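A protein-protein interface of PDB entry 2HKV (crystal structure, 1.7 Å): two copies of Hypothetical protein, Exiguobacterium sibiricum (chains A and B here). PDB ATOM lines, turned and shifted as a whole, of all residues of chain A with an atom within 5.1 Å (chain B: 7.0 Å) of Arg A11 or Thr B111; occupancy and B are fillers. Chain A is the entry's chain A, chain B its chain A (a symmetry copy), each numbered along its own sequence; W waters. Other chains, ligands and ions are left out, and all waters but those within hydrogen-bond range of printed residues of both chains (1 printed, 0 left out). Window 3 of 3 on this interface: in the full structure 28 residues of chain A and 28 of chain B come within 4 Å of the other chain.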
ATOM      1  N   GLN A   6       8.635 -15.379  19.567  1.00  0.00           N
ATOM      2  CA  GLN A   6       7.807 -14.839  20.646  1.00  0.00           C
ATOM      3  C   GLN A   6       7.547 -13.356  20.451  1.00  0.00           C
ATOM      4  O   GLN A   6       6.425 -12.867  20.700  1.00  0.00           O
ATOM      5  CB  GLN A   6       8.448 -15.041  22.003  1.00  0.00           C
ATOM      6  CG  GLN A   6       8.458 -16.530  22.452  1.00  0.00           C
ATOM      7  CD  GLN A   6       9.447 -16.886  23.548  1.00  0.00           C
ATOM      8  OE1 GLN A   6      10.493 -16.288  23.723  1.00  0.00           O
ATOM      9  NE2 GLN A   6       9.106 -17.942  24.256  1.00  0.00           N
ATOM     10  N   GLN A   7       8.590 -12.632  20.018  1.00  0.00           N
ATOM     11  CA  GLN A   7       8.460 -11.207  19.691  1.00  0.00           C
ATOM     12  C   GLN A   7       7.427 -10.978  18.597  1.00  0.00           C
ATOM     13  O   GLN A   7       6.595 -10.066  18.686  1.00  0.00           O
ATOM     14  CB  GLN A   7       9.808 -10.674  19.226  1.00  0.00           C
ATOM     15  CG  GLN A   7       9.768  -9.266  18.765  1.00  0.00           C
ATOM     16  CD  GLN A   7      11.164  -8.716  18.312  1.00  0.00           C
ATOM     17  OE1 GLN A   7      11.939  -9.351  17.550  1.00  0.00           O
ATOM     18  NE2 GLN A   7      11.486  -7.525  18.813  1.00  0.00           N
ATOM     19  N   ALA A   8       7.468 -11.819  17.574  1.00  0.00           N
ATOM     20  CA  ALA A   8       6.565 -11.727  16.409  1.00  0.00           C
ATOM     21  C   ALA A   8       5.125 -11.975  16.832  1.00  0.00           C
ATOM     22  O   ALA A   8       4.198 -11.241  16.474  1.00  0.00           O
ATOM     23  CB  ALA A   8       6.945 -12.724  15.432  1.00  0.00           C
ATOM     24  N   LEU A   9       4.936 -13.023  17.633  1.00  0.00           N
ATOM     25  CA  LEU A   9       3.603 -13.305  18.131  1.00  0.00           C
ATOM     26  C   LEU A   9       3.075 -12.183  19.026  1.00  0.00           C
ATOM     27  O   LEU A   9       1.922 -11.822  18.882  1.00  0.00           O
ATOM     28  CB  LEU A   9       3.499 -14.666  18.808  1.00  0.00           C
ATOM     29  CG  LEU A   9       3.435 -15.908  17.921  1.00  0.00           C
ATOM     30  CD1 LEU A   9       3.639 -17.213  18.746  1.00  0.00           C
ATOM     31  CD2 LEU A   9       2.150 -15.905  17.077  1.00  0.00           C
ATOM     32  N   ASP A  10       3.886 -11.693  19.966  1.00  0.00           N
ATOM     33  CA  ASP A  10       3.464 -10.607  20.849  1.00  0.00           C
ATOM     34  C   ASP A  10       3.038  -9.385  19.991  1.00  0.00           C
ATOM     35  O   ASP A  10       2.008  -8.741  20.240  1.00  0.00           O
ATOM     36  CB  ASP A  10       4.570 -10.269  21.825  1.00  0.00           C
ATOM     37  CG  ASP A  10       4.155  -9.250  22.853  1.00  0.00           C
ATOM     38  OD1 ASP A  10       3.218  -9.537  23.603  1.00  0.00           O
ATOM     39  OD2 ASP A  10       4.757  -8.151  22.903  1.00  0.00           O
ATOM     40  N   ARG A  11       3.804  -9.100  18.960  1.00  0.00           N
ATOM     41  CA  ARG A  11       3.497  -7.948  18.061  1.00  0.00           C
ATOM     42  C   ARG A  11       2.160  -8.127  17.323  1.00  0.00           C
ATOM     43  O   ARG A  11       1.262  -7.287  17.409  1.00  0.00           O
ATOM     44  CB  ARG A  11       4.646  -7.748  17.081  1.00  0.00           C
ATOM     45  CG  ARG A  11       4.415  -6.676  16.024  1.00  0.00           C
ATOM     46  CD  ARG A  11       5.659  -6.343  15.264  1.00  0.00           C
ATOM     47  NE  ARG A  11       5.386  -5.397  14.169  1.00  0.00           N
ATOM     48  CZ  ARG A  11       6.331  -4.692  13.540  1.00  0.00           C
ATOM     49  NH1 ARG A  11       7.582  -4.815  13.869  1.00  0.00           N
ATOM     50  NH2 ARG A  11       5.984  -3.836  12.572  1.00  0.00           N
ATOM     51  N   HIS A  12       2.058  -9.223  16.582  1.00  0.00           N
ATOM     52  CA  HIS A  12       0.950  -9.457  15.673  1.00  0.00           C
ATOM     53  C   HIS A  12      -0.300  -9.891  16.388  1.00  0.00           C
ATOM     54  O   HIS A  12      -1.415  -9.456  16.031  1.00  0.00           O
ATOM     55  CB  HIS A  12       1.390 -10.402  14.521  1.00  0.00           C
ATOM     56  CG  HIS A  12       2.387  -9.769  13.603  1.00  0.00           C
ATOM     57  ND1 HIS A  12       2.009  -8.893  12.588  1.00  0.00           N
ATOM     58  CD2 HIS A  12       3.739  -9.809  13.578  1.00  0.00           C
ATOM     59  CE1 HIS A  12       3.098  -8.416  12.008  1.00  0.00           C
ATOM     60  NE2 HIS A  12       4.160  -8.933  12.593  1.00  0.00           N
ATOM     61  N   VAL A  13      -0.184 -10.701  17.436  1.00  0.00           N
ATOM     62  CA  VAL A  13      -1.375 -11.000  18.224  1.00  0.00           C
ATOM     63  C   VAL A  13      -1.833  -9.749  19.004  1.00  0.00           C
ATOM     64  O   VAL A  13      -3.022  -9.474  19.129  1.00  0.00           O
ATOM     65  CB  VAL A  13      -1.235 -12.231  19.176  1.00  0.00           C
ATOM     66  CG1 VAL A  13      -2.558 -12.435  19.901  1.00  0.00           C
ATOM     67  CG2 VAL A  13      -0.878 -13.503  18.425  1.00  0.00           C
ATOM     68  N   GLY A  14      -0.898  -8.945  19.488  1.00  0.00           N
ATOM     69  CA  GLY A  14      -1.276  -7.667  20.139  1.00  0.00           C
ATOM     70  C   GLY A  14      -2.043  -6.728  19.196  1.00  0.00           C
ATOM     71  O   GLY A  14      -2.997  -6.038  19.608  1.00  0.00           O
ATOM     72  N   VAL A  15      -1.634  -6.658  17.929  1.00  0.00           N
ATOM     73  CA  VAL A  15      -2.379  -5.859  16.954  1.00  0.00           C
ATOM     74  C   VAL A  15      -3.771  -6.406  16.824  1.00  0.00           C
ATOM     75  O   VAL A  15      -4.747  -5.654  16.803  1.00  0.00           O
ATOM     76  CB  VAL A  15      -1.769  -5.874  15.496  1.00  0.00           C
ATOM     77  CG1 VAL A  15      -2.733  -5.256  14.489  1.00  0.00           C
ATOM     78  CG2 VAL A  15      -0.363  -5.185  15.407  1.00  0.00           C
ATOM     79  N   ARG A  18      -5.742  -5.446  19.965  1.00  0.00           N
ATOM     80  CA  ARG A  18      -6.127  -4.042  20.079  1.00  0.00           C
ATOM     81  C   ARG A  18      -7.153  -3.589  19.040  1.00  0.00           C
ATOM     82  O   ARG A  18      -8.086  -2.823  19.362  1.00  0.00           O
ATOM     83  CB  ARG A  18      -4.932  -3.141  20.041  1.00  0.00           C
ATOM     84  CG  ARG A  18      -4.066  -3.365  21.267  1.00  0.00           C
ATOM     85  CD  ARG A  18      -2.957  -2.375  21.373  1.00  0.00           C
ATOM     86  NE  ARG A  18      -2.156  -2.390  20.166  1.00  0.00           N
ATOM     87  CZ  ARG A  18      -1.036  -3.089  19.982  1.00  0.00           C
ATOM     88  NH1 ARG A  18      -0.518  -3.884  20.945  1.00  0.00           N
ATOM     89  NH2 ARG A  18      -0.434  -2.984  18.792  1.00  0.00           N
ATOM     90  N   THR B 103      15.347  -8.630   5.637  1.00  0.00           N
ATOM     91  CA  THR B 103      14.249  -7.666   5.508  1.00  0.00           C
ATOM     92  C   THR B 103      14.816  -6.263   5.520  1.00  0.00           C
ATOM     93  O   THR B 103      15.927  -6.015   5.991  1.00  0.00           O
ATOM     94  CB  THR B 103      13.173  -7.801   6.624  1.00  0.00           C
ATOM     95  OG1 THR B 103      13.779  -7.684   7.921  1.00  0.00           O
ATOM     96  CG2 THR B 103      12.467  -9.133   6.523  1.00  0.00           C
ATOM     97  N   GLU B 104      14.043  -5.362   4.955  1.00  0.00           N
ATOM     98  CA  GLU B 104      14.351  -3.954   4.911  1.00  0.00           C
ATOM     99  C   GLU B 104      13.085  -3.183   5.295  1.00  0.00           C
ATOM    100  O   GLU B 104      11.957  -3.695   5.196  1.00  0.00           O
ATOM    101  CB  GLU B 104      14.784  -3.568   3.498  1.00  0.00           C
ATOM    102  CG  GLU B 104      15.965  -4.399   2.952  1.00  0.00           C
ATOM    103  N   THR B 105      13.266  -1.943   5.724  1.00  0.00           N
ATOM    104  CA  THR B 105      12.114  -1.077   5.999  1.00  0.00           C
ATOM    105  C   THR B 105      11.329  -0.911   4.709  1.00  0.00           C
ATOM    106  O   THR B 105      11.918  -0.695   3.647  1.00  0.00           O
ATOM    107  CB  THR B 105      12.580   0.283   6.535  1.00  0.00           C
ATOM    108  OG1 THR B 105      13.290   0.071   7.773  1.00  0.00           O
ATOM    109  CG2 THR B 105      11.398   1.247   6.719  1.00  0.00           C
ATOM    110  N   THR B 106      10.010  -1.037   4.781  1.00  0.00           N
ATOM    111  CA  THR B 106       9.192  -0.978   3.580  1.00  0.00           C
ATOM    112  C   THR B 106       9.228   0.445   2.997  1.00  0.00           C
ATOM    113  O   THR B 106       9.743   1.401   3.626  1.00  0.00           O
ATOM    114  CB  THR B 106       7.719  -1.444   3.807  1.00  0.00           C
ATOM    115  OG1 THR B 106       6.929  -0.399   4.415  1.00  0.00           O
ATOM    116  CG2 THR B 106       7.675  -2.698   4.647  1.00  0.00           C
ATOM    117  N   GLY B 109       7.308   2.449   4.965  1.00  0.00           N
ATOM    118  CA  GLY B 109       8.072   2.625   6.217  1.00  0.00           C
ATOM    119  C   GLY B 109       7.810   1.647   7.371  1.00  0.00           C
ATOM    120  O   GLY B 109       8.230   1.915   8.508  1.00  0.00           O
ATOM    121  N   VAL B 110       7.160   0.511   7.115  1.00  0.00           N
ATOM    122  CA  VAL B 110       6.993  -0.489   8.199  1.00  0.00           C
ATOM    123  C   VAL B 110       8.255  -1.313   8.315  1.00  0.00           C
ATOM    124  O   VAL B 110       8.835  -1.708   7.287  1.00  0.00           O
ATOM    125  CB  VAL B 110       5.823  -1.396   8.009  1.00  0.00           C
ATOM    126  CG1 VAL B 110       5.879  -2.546   9.036  1.00  0.00           C
ATOM    127  CG2 VAL B 110       4.556  -0.614   8.189  1.00  0.00           C
ATOM    128  N   THR B 111       8.716  -1.474   9.560  1.00  0.00           N
ATOM    129  CA  THR B 111       9.887  -2.284   9.878  1.00  0.00           C
ATOM    130  C   THR B 111       9.466  -3.516  10.702  1.00  0.00           C
ATOM    131  O   THR B 111       8.635  -3.402  11.594  1.00  0.00           O
ATOM    132  CB  THR B 111      10.915  -1.467  10.666  1.00  0.00           C
ATOM    133  OG1 THR B 111      11.140  -0.201   9.996  1.00  0.00           O
ATOM    134  CG2 THR B 111      12.228  -2.228  10.765  1.00  0.00           C
ATOM    135  N   ASP B 112      10.000  -4.688  10.370  1.00  0.00           N
ATOM    136  CA  ASP B 112       9.720  -5.932  11.133  1.00  0.00           C
ATOM    137  C   ASP B 112      10.831  -6.896  10.803  1.00  0.00           C
ATOM    138  O   ASP B 112      11.533  -6.733   9.796  1.00  0.00           O
ATOM    139  CB  ASP B 112       8.338  -6.504  10.762  1.00  0.00           C
ATOM    140  CG  ASP B 112       7.763  -7.497  11.813  1.00  0.00           C
ATOM    141  OD1 ASP B 112       8.480  -7.853  12.802  1.00  0.00           O
ATOM    142  OD2 ASP B 112       6.572  -7.873  11.585  1.00  0.00           O
ATOM    143  N   SER B 113      11.024  -7.870  11.689  1.00  0.00           N
ATOM    144  CA  SER B 113      11.987  -8.944  11.491  1.00  0.00           C
ATOM    145  C   SER B 113      11.543  -9.904  10.399  1.00  0.00           C
ATOM    146  O   SER B 113      10.402  -9.857   9.972  1.00  0.00           O
ATOM    147  CB  SER B 113      12.144  -9.720  12.784  1.00  0.00           C
ATOM    148  OG  SER B 113      10.953 -10.385  13.124  1.00  0.00           O
ATOM    149  N   GLY B 116       8.811 -11.921  11.959  1.00  0.00           N
ATOM    150  CA  GLY B 116       7.593 -11.128  11.959  1.00  0.00           C
ATOM    151  C   GLY B 116       6.904 -11.001  10.616  1.00  0.00           C
ATOM    152  O   GLY B 116       5.698 -11.163  10.538  1.00  0.00           O
ATOM    153  N   TRP B 117       7.647 -10.796   9.550  1.00  0.00           N
ATOM    154  CA  TRP B 117       7.054 -10.759   8.222  1.00  0.00           C
ATOM    155  C   TRP B 117       6.449 -12.084   7.780  1.00  0.00           C
ATOM    156  O   TRP B 117       5.397 -12.121   7.158  1.00  0.00           O
ATOM    157  CB  TRP B 117       8.073 -10.265   7.172  1.00  0.00           C
ATOM    158  CG  TRP B 117       8.235  -8.759   7.157  1.00  0.00           C
ATOM    159  CD1 TRP B 117       9.341  -8.033   7.529  1.00  0.00           C
ATOM    160  CD2 TRP B 117       7.240  -7.800   6.749  1.00  0.00           C
ATOM    161  NE1 TRP B 117       9.080  -6.679   7.379  1.00  0.00           N
ATOM    162  CE2 TRP B 117       7.805  -6.513   6.915  1.00  0.00           C
ATOM    163  CE3 TRP B 117       5.932  -7.911   6.275  1.00  0.00           C
ATOM    164  CZ2 TRP B 117       7.113  -5.357   6.611  1.00  0.00           C
ATOM    165  CZ3 TRP B 117       5.243  -6.739   5.956  1.00  0.00           C
ATOM    166  CH2 TRP B 117       5.860  -5.486   6.122  1.00  0.00           C
ATOM    167  N   LEU B 119       5.207 -14.281   9.816  1.00  0.00           N
ATOM    168  CA  LEU B 119       3.936 -14.354  10.550  1.00  0.00           C
ATOM    169  C   LEU B 119       2.888 -13.378   9.975  1.00  0.00           C
ATOM    170  O   LEU B 119       1.686 -13.732   9.882  1.00  0.00           O
ATOM    171  CB  LEU B 119       4.135 -14.103  12.048  1.00  0.00           C
ATOM    172  CG  LEU B 119       2.883 -14.015  12.947  1.00  0.00           C
ATOM    173  CD1 LEU B 119       2.018 -15.277  12.831  1.00  0.00           C
ATOM    174  CD2 LEU B 119       3.348 -13.760  14.395  1.00  0.00           C
HETATM  175  O   HOH W   1      10.468 -10.859  15.801  1.00  0.00           O
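The backbone carbonyl oxygen (O) of Thr B111 lies within hydrogen-bond range of the guanidinium group (NH2) of Arg A11, at 2.9 Å. The guanidinium group (NH1) of Arg A11 lies within salt-bridge range of the side-chain carboxylate (OD1) of Asp B112 (3.3 Å). OD2 of Asp B112 is in hydrogen-bond range of NE2 of His A12 (2.8 Å). NE2 of His A12 sits at hydrogen-bond distance from O of Gly B116, at 3.4 Å.
OG1 of Thr B103 sits at hydrogen-bond distance from O of Asp B112 (3.1 Å). OG1 of Thr B111 lies within hydrogen-bond range of OG1 of Thr B105, at 3.1 Å. OG1 of Thr B106 is in hydrogen-bond range of N of Val B110. The backbone carbonyl oxygen (O) of Asp B112 lies close to the indole nitrogen (NE1) of Trp B117 (3.4 Å). The side-chain hydroxyl (OG) of Ser B113 is in hydrogen-bond range of the backbone NH (N) of Gly B116 (2.9 Å).
Among the printed residues, merely in contact across the chains: Ala A8 with Leu B119 (3.4 Å), Leu A9 with Leu B119 (3.6 Å), Arg A11 with Val B110 (3.8 Å), Ala A8 with Gly B116 (3.9 Å) and His A12 with Leu B119 (3.9 Å).
Of chain A, only Arg A11 (2.9 Å) comes within 4 Å of Thr B111. Of the printed residues of chain B, Ala A8 touches Gly B116 and Leu B119. Of the printed residues of chain A, Gly B116 touches Ala A8 (3.9 Å) and His A12 (3.4 Å). Printed residues of chain A within 4 Å of Asp B112: Arg A11 and His A12. Printed residues of chain A within 4 Å of Val B110: Arg A11 (3.8 Å). Of the printed residues of chain A, Leu B119 touches Ala A8 (3.4 Å), Leu A9 (3.6 Å) and His A12 (3.9 Å). Glu B104 touches none of the printed residues of chain A. Arg A18 touches none of the printed residues of chain B. The nearest printed residue of chain A that does not touch Thr B111 is His A12 (7.2 Å). The nearest printed residue of chain A that does not touch Gly B116 is Arg A11 (6.1 Å).
Hydrophobic or aromatic side chains of chain B that line the printed part of chain A: Val B110 and Leu B119. Of the 11 printed residues of chain A, 4 touch a printed residue of chain B. Hydrophobic or aromatic side chains of chain A within 4 Å of the printed part of chain B: Ala A8, Leu A9 and His A12. Among the printed residues, Asp or Glu carboxylates within 4 Å of a Lys or Arg side-chain nitrogen of the other chain: Arg A11 with Asp B112 (3.3 Å).
No position is printed for both chains.
Water W1 bridges the side-chain amide oxygen of Gln A7 (2.7 Å) and the side-chain hydroxyl of Ser B113 (2.8 Å).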
